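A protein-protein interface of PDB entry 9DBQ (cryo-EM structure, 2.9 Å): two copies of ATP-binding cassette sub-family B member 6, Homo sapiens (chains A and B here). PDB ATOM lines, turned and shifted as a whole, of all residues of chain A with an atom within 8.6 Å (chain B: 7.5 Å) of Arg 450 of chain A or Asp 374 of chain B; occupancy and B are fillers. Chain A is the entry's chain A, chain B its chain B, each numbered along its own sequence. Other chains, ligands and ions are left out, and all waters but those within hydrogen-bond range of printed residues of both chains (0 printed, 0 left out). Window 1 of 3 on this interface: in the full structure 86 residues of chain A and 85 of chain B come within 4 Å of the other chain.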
ATOM      1  N   ASN A 443      -3.852   1.314   2.389  1.00  0.00           N
ATOM      2  CA  ASN A 443      -3.418   1.148   3.772  1.00  0.00           C
ATOM      3  C   ASN A 443      -3.907  -0.172   4.349  1.00  0.00           C
ATOM      4  O   ASN A 443      -3.155  -0.870   5.038  1.00  0.00           O
ATOM      5  CB  ASN A 443      -3.919   2.312   4.620  1.00  0.00           C
ATOM      6  CG  ASN A 443      -3.640   3.654   3.986  1.00  0.00           C
ATOM      7  OD1 ASN A 443      -2.531   3.918   3.525  1.00  0.00           O
ATOM      8  ND2 ASN A 443      -4.655   4.509   3.947  1.00  0.00           N
ATOM      9  N   THR A 444      -5.161  -0.536   4.073  1.00  0.00           N
ATOM     10  CA  THR A 444      -5.699  -1.776   4.623  1.00  0.00           C
ATOM     11  C   THR A 444      -4.920  -2.982   4.117  1.00  0.00           C
ATOM     12  O   THR A 444      -4.600  -3.893   4.890  1.00  0.00           O
ATOM     13  CB  THR A 444      -7.176  -1.917   4.265  1.00  0.00           C
ATOM     14  OG1 THR A 444      -7.314  -2.057   2.846  1.00  0.00           O
ATOM     15  CG2 THR A 444      -7.960  -0.699   4.734  1.00  0.00           C
ATOM     16  N   GLN A 445      -4.595  -3.002   2.825  1.00  0.00           N
ATOM     17  CA  GLN A 445      -3.807  -4.103   2.281  1.00  0.00           C
ATOM     18  C   GLN A 445      -2.413  -4.135   2.896  1.00  0.00           C
ATOM     19  O   GLN A 445      -1.882  -5.211   3.188  1.00  0.00           O
ATOM     20  CB  GLN A 445      -3.725  -3.982   0.762  1.00  0.00           C
ATOM     21  CG  GLN A 445      -3.027  -5.143   0.086  1.00  0.00           C
ATOM     22  CD  GLN A 445      -3.682  -6.469   0.399  1.00  0.00           C
ATOM     23  OE1 GLN A 445      -4.906  -6.594   0.358  1.00  0.00           O
ATOM     24  NE2 GLN A 445      -2.872  -7.463   0.729  1.00  0.00           N
ATOM     25  N   GLU A 446      -1.809  -2.964   3.106  1.00  0.00           N
ATOM     26  CA  GLU A 446      -0.484  -2.919   3.715  1.00  0.00           C
ATOM     27  C   GLU A 446      -0.513  -3.510   5.117  1.00  0.00           C
ATOM     28  O   GLU A 446       0.400  -4.244   5.511  1.00  0.00           O
ATOM     29  CB  GLU A 446       0.026  -1.480   3.749  1.00  0.00           C
ATOM     30  CG  GLU A 446       1.501  -1.350   4.106  1.00  0.00           C
ATOM     31  CD  GLU A 446       1.735  -1.159   5.596  1.00  0.00           C
ATOM     32  OE1 GLU A 446       0.871  -0.563   6.273  1.00  0.00           O
ATOM     33  OE2 GLU A 446       2.791  -1.606   6.092  1.00  0.00           O
ATOM     34  N   ASN A 447      -1.558  -3.203   5.886  1.00  0.00           N
ATOM     35  CA  ASN A 447      -1.688  -3.786   7.215  1.00  0.00           C
ATOM     36  C   ASN A 447      -1.924  -5.289   7.151  1.00  0.00           C
ATOM     37  O   ASN A 447      -1.458  -6.026   8.026  1.00  0.00           O
ATOM     38  CB  ASN A 447      -2.826  -3.102   7.970  1.00  0.00           C
ATOM     39  CG  ASN A 447      -2.541  -1.644   8.251  1.00  0.00           C
ATOM     40  OD1 ASN A 447      -1.415  -1.273   8.577  1.00  0.00           O
ATOM     41  ND2 ASN A 447      -3.562  -0.806   8.118  1.00  0.00           N
ATOM     42  N   ALA A 448      -2.643  -5.761   6.131  1.00  0.00           N
ATOM     43  CA  ALA A 448      -2.933  -7.187   6.033  1.00  0.00           C
ATOM     44  C   ALA A 448      -1.696  -7.994   5.659  1.00  0.00           C
ATOM     45  O   ALA A 448      -1.536  -9.127   6.126  1.00  0.00           O
ATOM     46  CB  ALA A 448      -4.044  -7.427   5.013  1.00  0.00           C
ATOM     47  N   THR A 449      -0.819  -7.440   4.820  1.00  0.00           N
ATOM     48  CA  THR A 449       0.351  -8.189   4.370  1.00  0.00           C
ATOM     49  C   THR A 449       1.316  -8.451   5.519  1.00  0.00           C
ATOM     50  O   THR A 449       1.745  -9.589   5.735  1.00  0.00           O
ATOM     51  CB  THR A 449       1.055  -7.430   3.247  1.00  0.00           C
ATOM     52  OG1 THR A 449       0.149  -7.236   2.155  1.00  0.00           O
ATOM     53  CG2 THR A 449       2.271  -8.202   2.761  1.00  0.00           C
ATOM     54  N   ARG A 450       1.666  -7.408   6.273  1.00  0.00           N
ATOM     55  CA  ARG A 450       2.642  -7.576   7.345  1.00  0.00           C
ATOM     56  C   ARG A 450       2.099  -8.450   8.465  1.00  0.00           C
ATOM     57  O   ARG A 450       2.876  -9.117   9.157  1.00  0.00           O
ATOM     58  CB  ARG A 450       3.062  -6.213   7.890  1.00  0.00           C
ATOM     59  CG  ARG A 450       3.898  -5.398   6.920  1.00  0.00           C
ATOM     60  CD  ARG A 450       4.425  -4.119   7.548  1.00  0.00           C
ATOM     61  NE  ARG A 450       5.222  -3.340   6.605  1.00  0.00           N
ATOM     62  CZ  ARG A 450       5.774  -2.165   6.878  1.00  0.00           C
ATOM     63  NH1 ARG A 450       5.637  -1.595   8.064  1.00  0.00           N
ATOM     64  NH2 ARG A 450       6.480  -1.548   5.936  1.00  0.00           N
ATOM     65  N   ALA A 451       0.781  -8.464   8.664  1.00  0.00           N
ATOM     66  CA  ALA A 451       0.201  -9.330   9.685  1.00  0.00           C
ATOM     67  C   ALA A 451       0.476 -10.794   9.375  1.00  0.00           C
ATOM     68  O   ALA A 451       0.820 -11.577  10.266  1.00  0.00           O
ATOM     69  CB  ALA A 451      -1.301  -9.073   9.802  1.00  0.00           C
ATOM     70  N   ARG A 452       0.323 -11.186   8.109  1.00  0.00           N
ATOM     71  CA  ARG A 452       0.655 -12.552   7.721  1.00  0.00           C
ATOM     72  C   ARG A 452       2.148 -12.817   7.872  1.00  0.00           C
ATOM     73  O   ARG A 452       2.555 -13.906   8.289  1.00  0.00           O
ATOM     74  CB  ARG A 452       0.207 -12.813   6.283  1.00  0.00           C
ATOM     75  CG  ARG A 452       0.576 -14.192   5.747  1.00  0.00           C
ATOM     76  CD  ARG A 452       0.022 -15.303   6.624  1.00  0.00           C
ATOM     77  NE  ARG A 452       0.386 -16.626   6.128  1.00  0.00           N
ATOM     78  CZ  ARG A 452      -0.308 -17.314   5.232  1.00  0.00           C
ATOM     79  NH1 ARG A 452      -1.409 -16.826   4.683  1.00  0.00           N
ATOM     80  NH2 ARG A 452       0.114 -18.522   4.878  1.00  0.00           N
ATOM     81  N   ALA A 453       2.981 -11.833   7.527  1.00  0.00           N
ATOM     82  CA  ALA A 453       4.426 -12.011   7.636  1.00  0.00           C
ATOM     83  C   ALA A 453       4.844 -12.258   9.079  1.00  0.00           C
ATOM     84  O   ALA A 453       5.590 -13.200   9.367  1.00  0.00           O
ATOM     85  CB  ALA A 453       5.146 -10.787   7.073  1.00  0.00           C
ATOM     86  N   VAL A 454       4.369 -11.422  10.004  1.00  0.00           N
ATOM     87  CA  VAL A 454       4.792 -11.548  11.394  1.00  0.00           C
ATOM     88  C   VAL A 454       4.203 -12.802  12.027  1.00  0.00           C
ATOM     89  O   VAL A 454       4.838 -13.427  12.884  1.00  0.00           O
ATOM     90  CB  VAL A 454       4.417 -10.280  12.182  1.00  0.00           C
ATOM     91  CG1 VAL A 454       2.915 -10.215  12.426  1.00  0.00           C
ATOM     92  CG2 VAL A 454       5.187 -10.220  13.490  1.00  0.00           C
ATOM     93  N   ASP A 455       2.996 -13.201  11.619  1.00  0.00           N
ATOM     94  CA  ASP A 455       2.438 -14.454  12.116  1.00  0.00           C
ATOM     95  C   ASP A 455       3.231 -15.650  11.609  1.00  0.00           C
ATOM     96  O   ASP A 455       3.331 -16.665  12.304  1.00  0.00           O
ATOM     97  CB  ASP A 455       0.973 -14.580  11.708  1.00  0.00           C
ATOM     98  CG  ASP A 455       0.062 -13.665  12.501  1.00  0.00           C
ATOM     99  OD1 ASP A 455       0.452 -13.256  13.615  1.00  0.00           O
ATOM    100  OD2 ASP A 455      -1.045 -13.356  12.015  1.00  0.00           O
ATOM    101  N   SER A 456       3.792 -15.550  10.404  1.00  0.00           N
ATOM    102  CA  SER A 456       4.630 -16.624   9.883  1.00  0.00           C
ATOM    103  C   SER A 456       5.889 -16.791  10.724  1.00  0.00           C
ATOM    104  O   SER A 456       6.303 -17.915  11.030  1.00  0.00           O
ATOM    105  CB  SER A 456       4.991 -16.338   8.425  1.00  0.00           C
ATOM    106  OG  SER A 456       5.893 -17.307   7.924  1.00  0.00           O
ATOM    107  N   LEU A 457       6.518 -15.677  11.099  1.00  0.00           N
ATOM    108  CA  LEU A 457       7.780 -15.731  11.828  1.00  0.00           C
ATOM    109  C   LEU A 457       7.588 -16.037  13.309  1.00  0.00           C
ATOM    110  O   LEU A 457       8.484 -16.611  13.935  1.00  0.00           O
ATOM    111  CB  LEU A 457       8.530 -14.409  11.661  1.00  0.00           C
ATOM    112  CG  LEU A 457       9.542 -14.349  10.518  1.00  0.00           C
ATOM    113  CD1 LEU A 457       9.978 -12.915  10.271  1.00  0.00           C
ATOM    114  CD2 LEU A 457      10.739 -15.227  10.821  1.00  0.00           C
ATOM    115  N   TYR A 476       3.861 -15.112   1.257  1.00  0.00           N
ATOM    116  CA  TYR A 476       4.301 -13.732   1.426  1.00  0.00           C
ATOM    117  C   TYR A 476       4.491 -13.055   0.077  1.00  0.00           C
ATOM    118  O   TYR A 476       4.187 -11.868  -0.080  1.00  0.00           O
ATOM    119  CB  TYR A 476       5.592 -13.692   2.239  1.00  0.00           C
ATOM    120  CG  TYR A 476       5.999 -12.313   2.700  1.00  0.00           C
ATOM    121  CD1 TYR A 476       5.055 -11.393   3.129  1.00  0.00           C
ATOM    122  CD2 TYR A 476       7.333 -11.943   2.729  1.00  0.00           C
ATOM    123  CE1 TYR A 476       5.430 -10.138   3.555  1.00  0.00           C
ATOM    124  CE2 TYR A 476       7.715 -10.693   3.158  1.00  0.00           C
ATOM    125  CZ  TYR A 476       6.760  -9.794   3.572  1.00  0.00           C
ATOM    126  OH  TYR A 476       7.133  -8.541   4.001  1.00  0.00           O
ATOM    127  N   ALA A 479       0.981 -12.057  -1.247  1.00  0.00           N
ATOM    128  CA  ALA A 479       0.455 -10.898  -0.536  1.00  0.00           C
ATOM    129  C   ALA A 479       1.183  -9.630  -0.955  1.00  0.00           C
ATOM    130  O   ALA A 479       0.565  -8.569  -1.100  1.00  0.00           O
ATOM    131  CB  ALA A 479       0.565 -11.107   0.972  1.00  0.00           C
ATOM    132  N   ILE A 480       2.499  -9.717  -1.150  1.00  0.00           N
ATOM    133  CA  ILE A 480       3.252  -8.569  -1.644  1.00  0.00           C
ATOM    134  C   ILE A 480       2.743  -8.156  -3.017  1.00  0.00           C
ATOM    135  O   ILE A 480       2.551  -6.967  -3.291  1.00  0.00           O
ATOM    136  CB  ILE A 480       4.758  -8.894  -1.665  1.00  0.00           C
ATOM    137  CG1 ILE A 480       5.334  -8.800  -0.251  1.00  0.00           C
ATOM    138  CG2 ILE A 480       5.505  -7.959  -2.604  1.00  0.00           C
ATOM    139  CD1 ILE A 480       6.778  -9.226  -0.144  1.00  0.00           C
ATOM    140  N   TYR A 483      -0.306  -6.103  -2.812  1.00  0.00           N
ATOM    141  CA  TYR A 483      -0.017  -4.766  -2.311  1.00  0.00           C
ATOM    142  C   TYR A 483       0.630  -3.909  -3.389  1.00  0.00           C
ATOM    143  O   TYR A 483       0.342  -2.713  -3.496  1.00  0.00           O
ATOM    144  CB  TYR A 483       0.881  -4.850  -1.083  1.00  0.00           C
ATOM    145  CG  TYR A 483       1.282  -3.507  -0.543  1.00  0.00           C
ATOM    146  CD1 TYR A 483       0.325  -2.570  -0.198  1.00  0.00           C
ATOM    147  CD2 TYR A 483       2.617  -3.180  -0.368  1.00  0.00           C
ATOM    148  CE1 TYR A 483       0.687  -1.339   0.299  1.00  0.00           C
ATOM    149  CE2 TYR A 483       2.990  -1.953   0.130  1.00  0.00           C
ATOM    150  CZ  TYR A 483       2.020  -1.036   0.464  1.00  0.00           C
ATOM    151  OH  TYR A 483       2.385   0.193   0.963  1.00  0.00           O
ATOM    152  N   SER B 342      12.122  -3.829  -4.698  1.00  0.00           N
ATOM    153  CA  SER B 342      11.626  -3.901  -3.328  1.00  0.00           C
ATOM    154  C   SER B 342      11.116  -5.299  -3.005  1.00  0.00           C
ATOM    155  O   SER B 342      11.343  -5.812  -1.906  1.00  0.00           O
ATOM    156  CB  SER B 342      10.524  -2.866  -3.117  1.00  0.00           C
ATOM    157  OG  SER B 342      10.006  -2.940  -1.801  1.00  0.00           O
ATOM    158  N   GLU B 346      12.864  -7.852  -0.224  1.00  0.00           N
ATOM    159  CA  GLU B 346      11.982  -8.313   0.844  1.00  0.00           C
ATOM    160  C   GLU B 346      11.995  -9.830   0.954  1.00  0.00           C
ATOM    161  O   GLU B 346      12.085 -10.379   2.056  1.00  0.00           O
ATOM    162  CB  GLU B 346      10.560  -7.820   0.591  1.00  0.00           C
ATOM    163  CG  GLU B 346      10.246  -6.464   1.187  1.00  0.00           C
ATOM    164  CD  GLU B 346       9.974  -6.533   2.676  1.00  0.00           C
ATOM    165  OE1 GLU B 346       9.913  -7.653   3.224  1.00  0.00           O
ATOM    166  OE2 GLU B 346       9.818  -5.463   3.301  1.00  0.00           O
ATOM    167  N   ILE B 349      15.392 -11.130   2.401  1.00  0.00           N
ATOM    168  CA  ILE B 349      15.495 -10.988   3.849  1.00  0.00           C
ATOM    169  C   ILE B 349      14.617 -12.017   4.547  1.00  0.00           C
ATOM    170  O   ILE B 349      15.048 -12.678   5.498  1.00  0.00           O
ATOM    171  CB  ILE B 349      15.126  -9.552   4.263  1.00  0.00           C
ATOM    172  CG1 ILE B 349      16.144  -8.563   3.688  1.00  0.00           C
ATOM    173  CG2 ILE B 349      15.046  -9.432   5.778  1.00  0.00           C
ATOM    174  CD1 ILE B 349      15.776  -7.111   3.886  1.00  0.00           C
ATOM    175  N   GLY B 367       9.581  -8.491  16.483  1.00  0.00           N
ATOM    176  CA  GLY B 367       8.971  -7.247  16.044  1.00  0.00           C
ATOM    177  C   GLY B 367       9.988  -6.232  15.563  1.00  0.00           C
ATOM    178  O   GLY B 367       9.820  -5.626  14.502  1.00  0.00           O
ATOM    179  N   GLU B 368      11.064  -6.038  16.328  1.00  0.00           N
ATOM    180  CA  GLU B 368      12.098  -5.095  15.913  1.00  0.00           C
ATOM    181  C   GLU B 368      12.832  -5.583  14.669  1.00  0.00           C
ATOM    182  O   GLU B 368      13.315  -4.764  13.878  1.00  0.00           O
ATOM    183  CB  GLU B 368      13.077  -4.854  17.063  1.00  0.00           C
ATOM    184  CG  GLU B 368      13.794  -6.105  17.557  1.00  0.00           C
ATOM    185  CD  GLU B 368      15.137  -6.332  16.882  1.00  0.00           C
ATOM    186  OE1 GLU B 368      15.672  -5.391  16.259  1.00  0.00           O
ATOM    187  OE2 GLU B 368      15.663  -7.461  16.980  1.00  0.00           O
ATOM    188  N   VAL B 369      12.921  -6.899  14.473  1.00  0.00           N
ATOM    189  CA  VAL B 369      13.569  -7.422  13.274  1.00  0.00           C
ATOM    190  C   VAL B 369      12.759  -7.063  12.036  1.00  0.00           C
ATOM    191  O   VAL B 369      13.314  -6.640  11.015  1.00  0.00           O
ATOM    192  CB  VAL B 369      13.780  -8.940  13.394  1.00  0.00           C
ATOM    193  CG1 VAL B 369      14.574  -9.464  12.210  1.00  0.00           C
ATOM    194  CG2 VAL B 369      14.489  -9.277  14.695  1.00  0.00           C
ATOM    195  N   LEU B 370      11.434  -7.217  12.104  1.00  0.00           N
ATOM    196  CA  LEU B 370      10.591  -6.798  10.989  1.00  0.00           C
ATOM    197  C   LEU B 370      10.724  -5.302  10.742  1.00  0.00           C
ATOM    198  O   LEU B 370      10.784  -4.856   9.591  1.00  0.00           O
ATOM    199  CB  LEU B 370       9.132  -7.161  11.261  1.00  0.00           C
ATOM    200  CG  LEU B 370       8.656  -8.554  10.842  1.00  0.00           C
ATOM    201  CD1 LEU B 370       8.766  -8.742   9.335  1.00  0.00           C
ATOM    202  CD2 LEU B 370       9.428  -9.632  11.581  1.00  0.00           C
ATOM    203  N   ARG B 371      10.774  -4.510  11.813  1.00  0.00           N
ATOM    204  CA  ARG B 371      10.940  -3.070  11.661  1.00  0.00           C
ATOM    205  C   ARG B 371      12.256  -2.742  10.968  1.00  0.00           C
ATOM    206  O   ARG B 371      12.305  -1.872  10.092  1.00  0.00           O
ATOM    207  CB  ARG B 371      10.854  -2.397  13.030  1.00  0.00           C
ATOM    208  CG  ARG B 371      10.722  -0.882  12.983  1.00  0.00           C
ATOM    209  CD  ARG B 371      12.062  -0.176  13.143  1.00  0.00           C
ATOM    210  NE  ARG B 371      12.803  -0.660  14.302  1.00  0.00           N
ATOM    211  CZ  ARG B 371      12.573  -0.290  15.555  1.00  0.00           C
ATOM    212  NH1 ARG B 371      11.615   0.570  15.861  1.00  0.00           N
ATOM    213  NH2 ARG B 371      13.322  -0.800  16.527  1.00  0.00           N
ATOM    214  N   ILE B 372      13.335  -3.432  11.344  1.00  0.00           N
ATOM    215  CA  ILE B 372      14.614  -3.231  10.669  1.00  0.00           C
ATOM    216  C   ILE B 372      14.514  -3.640   9.207  1.00  0.00           C
ATOM    217  O   ILE B 372      15.048  -2.966   8.319  1.00  0.00           O
ATOM    218  CB  ILE B 372      15.729  -4.006  11.397  1.00  0.00           C
ATOM    219  CG1 ILE B 372      16.032  -3.358  12.750  1.00  0.00           C
ATOM    220  CG2 ILE B 372      16.985  -4.078  10.539  1.00  0.00           C
ATOM    221  CD1 ILE B 372      16.513  -1.924  12.661  1.00  0.00           C
ATOM    222  N   ALA B 373      13.833  -4.753   8.931  1.00  0.00           N
ATOM    223  CA  ALA B 373      13.747  -5.242   7.560  1.00  0.00           C
ATOM    224  C   ALA B 373      13.025  -4.246   6.662  1.00  0.00           C
ATOM    225  O   ALA B 373      13.536  -3.872   5.602  1.00  0.00           O
ATOM    226  CB  ALA B 373      13.043  -6.599   7.530  1.00  0.00           C
ATOM    227  N   ASP B 374      11.838  -3.797   7.072  1.00  0.00           N
ATOM    228  CA  ASP B 374      11.080  -2.878   6.229  1.00  0.00           C
ATOM    229  C   ASP B 374      11.794  -1.539   6.092  1.00  0.00           C
ATOM    230  O   ASP B 374      11.809  -0.947   5.007  1.00  0.00           O
ATOM    231  CB  ASP B 374       9.673  -2.688   6.789  1.00  0.00           C
ATOM    232  CG  ASP B 374       9.674  -2.132   8.194  1.00  0.00           C
ATOM    233  OD1 ASP B 374      10.202  -1.020   8.400  1.00  0.00           O
ATOM    234  OD2 ASP B 374       9.137  -2.811   9.094  1.00  0.00           O
ATOM    235  N   ARG B 375      12.392  -1.045   7.177  1.00  0.00           N
ATOM    236  CA  ARG B 375      13.152   0.198   7.090  1.00  0.00           C
ATOM    237  C   ARG B 375      14.326   0.052   6.133  1.00  0.00           C
ATOM    238  O   ARG B 375      14.630   0.973   5.367  1.00  0.00           O
ATOM    239  CB  ARG B 375      13.641   0.622   8.474  1.00  0.00           C
ATOM    240  CG  ARG B 375      12.598   1.335   9.313  1.00  0.00           C
ATOM    241  CD  ARG B 375      13.230   2.043  10.497  1.00  0.00           C
ATOM    242  NE  ARG B 375      12.247   2.777  11.287  1.00  0.00           N
ATOM    243  CZ  ARG B 375      12.530   3.453  12.392  1.00  0.00           C
ATOM    244  NH1 ARG B 375      13.761   3.509  12.874  1.00  0.00           N
ATOM    245  NH2 ARG B 375      11.552   4.088  13.031  1.00  0.00           N
ATOM    246  N   GLY B 376      15.003  -1.097   6.164  1.00  0.00           N
ATOM    247  CA  GLY B 376      16.112  -1.308   5.250  1.00  0.00           C
ATOM    248  C   GLY B 376      15.677  -1.306   3.797  1.00  0.00           C
ATOM    249  O   GLY B 376      16.332  -0.701   2.945  1.00  0.00           O
ATOM    250  N   THR B 377      14.567  -1.982   3.491  1.00  0.00           N
ATOM    251  CA  THR B 377      14.096  -2.041   2.110  1.00  0.00           C
ATOM    252  C   THR B 377      13.662  -0.666   1.621  1.00  0.00           C
ATOM    253  O   THR B 377      14.002  -0.255   0.507  1.00  0.00           O
ATOM    254  CB  THR B 377      12.948  -3.040   1.986  1.00  0.00           C
ATOM    255  OG1 THR B 377      11.862  -2.629   2.825  1.00  0.00           O
ATOM    256  CG2 THR B 377      13.407  -4.432   2.395  1.00  0.00           C
ATOM    257  N   SER B 378      12.908   0.066   2.445  1.00  0.00           N
ATOM    258  CA  SER B 378      12.518   1.422   2.075  1.00  0.00           C
ATOM    259  C   SER B 378      13.740   2.320   1.938  1.00  0.00           C
ATOM    260  O   SER B 378      13.798   3.170   1.044  1.00  0.00           O
ATOM    261  CB  SER B 378      11.549   1.993   3.110  1.00  0.00           C
ATOM    262  OG  SER B 378      12.160   2.084   4.386  1.00  0.00           O
ATOM    263  N   SER B 379      14.725   2.147   2.821  1.00  0.00           N
ATOM    264  CA  SER B 379      15.949   2.933   2.726  1.00  0.00           C
ATOM    265  C   SER B 379      16.682   2.662   1.418  1.00  0.00           C
ATOM    266  O   SER B 379      17.180   3.591   0.773  1.00  0.00           O
ATOM    267  CB  SER B 379      16.855   2.628   3.917  1.00  0.00           C
ATOM    268  OG  SER B 379      18.135   3.211   3.747  1.00  0.00           O
ATOM    269  N   VAL B 380      16.762   1.394   1.010  1.00  0.00           N
ATOM    270  CA  VAL B 380      17.503   1.047  -0.200  1.00  0.00           C
ATOM    271  C   VAL B 380      16.856   1.683  -1.423  1.00  0.00           C
ATOM    272  O   VAL B 380      17.524   2.337  -2.233  1.00  0.00           O
ATOM    273  CB  VAL B 380      17.596  -0.480  -0.349  1.00  0.00           C
ATOM    274  CG1 VAL B 380      17.954  -0.856  -1.777  1.00  0.00           C
ATOM    275  CG2 VAL B 380      18.610  -1.045   0.627  1.00  0.00           C
ATOM    276  N   THR B 381      15.544   1.500  -1.577  1.00  0.00           N
ATOM    277  CA  THR B 381      14.864   2.038  -2.751  1.00  0.00           C
ATOM    278  C   THR B 381      14.855   3.561  -2.737  1.00  0.00           C
ATOM    279  O   THR B 381      15.064   4.197  -3.776  1.00  0.00           O
ATOM    280  CB  THR B 381      13.437   1.489  -2.835  1.00  0.00           C
ATOM    281  OG1 THR B 381      12.793   2.005  -4.005  1.00  0.00           O
ATOM    282  CG2 THR B 381      12.617   1.868  -1.605  1.00  0.00           C
ATOM    283  N   MET B 564      20.331  -2.944   8.264  1.00  0.00           N
ATOM    284  CA  MET B 564      19.819  -4.082   7.507  1.00  0.00           C
ATOM    285  C   MET B 564      20.946  -5.019   7.095  1.00  0.00           C
ATOM    286  O   MET B 564      20.824  -6.242   7.223  1.00  0.00           O
ATOM    287  CB  MET B 564      19.068  -3.589   6.271  1.00  0.00           C
ATOM    288  CG  MET B 564      18.541  -4.694   5.364  1.00  0.00           C
ATOM    289  SD  MET B 564      17.932  -4.070   3.786  1.00  0.00           S
ATOM    290  CE  MET B 564      19.428  -4.125   2.799  1.00  0.00           C
ATOM    291  N   LEU B 567      21.902  -7.067   9.889  1.00  0.00           N
ATOM    292  CA  LEU B 567      20.942  -8.146  10.096  1.00  0.00           C
ATOM    293  C   LEU B 567      21.219  -9.319   9.162  1.00  0.00           C
ATOM    294  O   LEU B 567      21.143 -10.482   9.575  1.00  0.00           O
ATOM    295  CB  LEU B 567      19.525  -7.617   9.895  1.00  0.00           C
ATOM    296  CG  LEU B 567      18.376  -8.612  10.027  1.00  0.00           C
ATOM    297  CD1 LEU B 567      18.365  -9.243  11.406  1.00  0.00           C
ATOM    298  CD2 LEU B 567      17.055  -7.920   9.738  1.00  0.00           C
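The side-chain carboxylate (OD2) of Asp 374 of chain B lies within salt-bridge range of the guanidinium group (NH1) of Arg 450 of chain A, at 3.8 Å. The side-chain carboxylate of Glu 346 of chain B lies within hydrogen-bond range of the side-chain hydroxyl of Tyr 476 of chain A.
OE2 of Glu 446 of chain A lies within salt-bridge range of NE of Arg 450 of chain A, at 3.0 Å. The backbone carbonyl oxygen (O) of Leu 370 of chain B sits close to the side-chain carboxylate (OD2) of Asp 374 of chain B (2.7 Å). The side-chain hydroxyl of Thr 377 of chain B is in hydrogen-bond range of the backbone carbonyl oxygen of Asp 374 of chain B. The backbone carbonyl oxygen of Asp 374 of chain B is in hydrogen-bond range of the side-chain hydroxyl of Ser 378 of chain B, 3.1 Å away.
Leu 457 of chain A touches Leu 370 of chain B.
Of chain B, only Asp 374 comes within 4 Å of Arg 450 of chain A. Of the printed residues of chain B, Leu 457 of chain A touches Leu 370. Of the printed residues of chain A, Glu 346 of chain B touches Tyr 476. Of the printed residues of chain A, Leu 370 of chain B touches Leu 457. No residue of chain A comes within 4 Å of Ala 373 of chain B. Asp 374 of chain B touches one residue of chain A. Gly 376 of chain B touches none of the printed residues of chain A.
Of the 19 printed residues of chain A, 3 touch a printed residue of chain B. Of the 20 printed residues of chain B, 3 touch a printed residue of chain A. Among the printed residues, Asp or Glu carboxylates within 4 Å of a Lys or Arg side-chain nitrogen of the other chain: Arg 450 of chain A with Asp 374 of chain B.
No position is printed for both chains. Of the 3 pairs that touch across the chains among the printed residues, none has its exchanged pair printed and touching as well.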
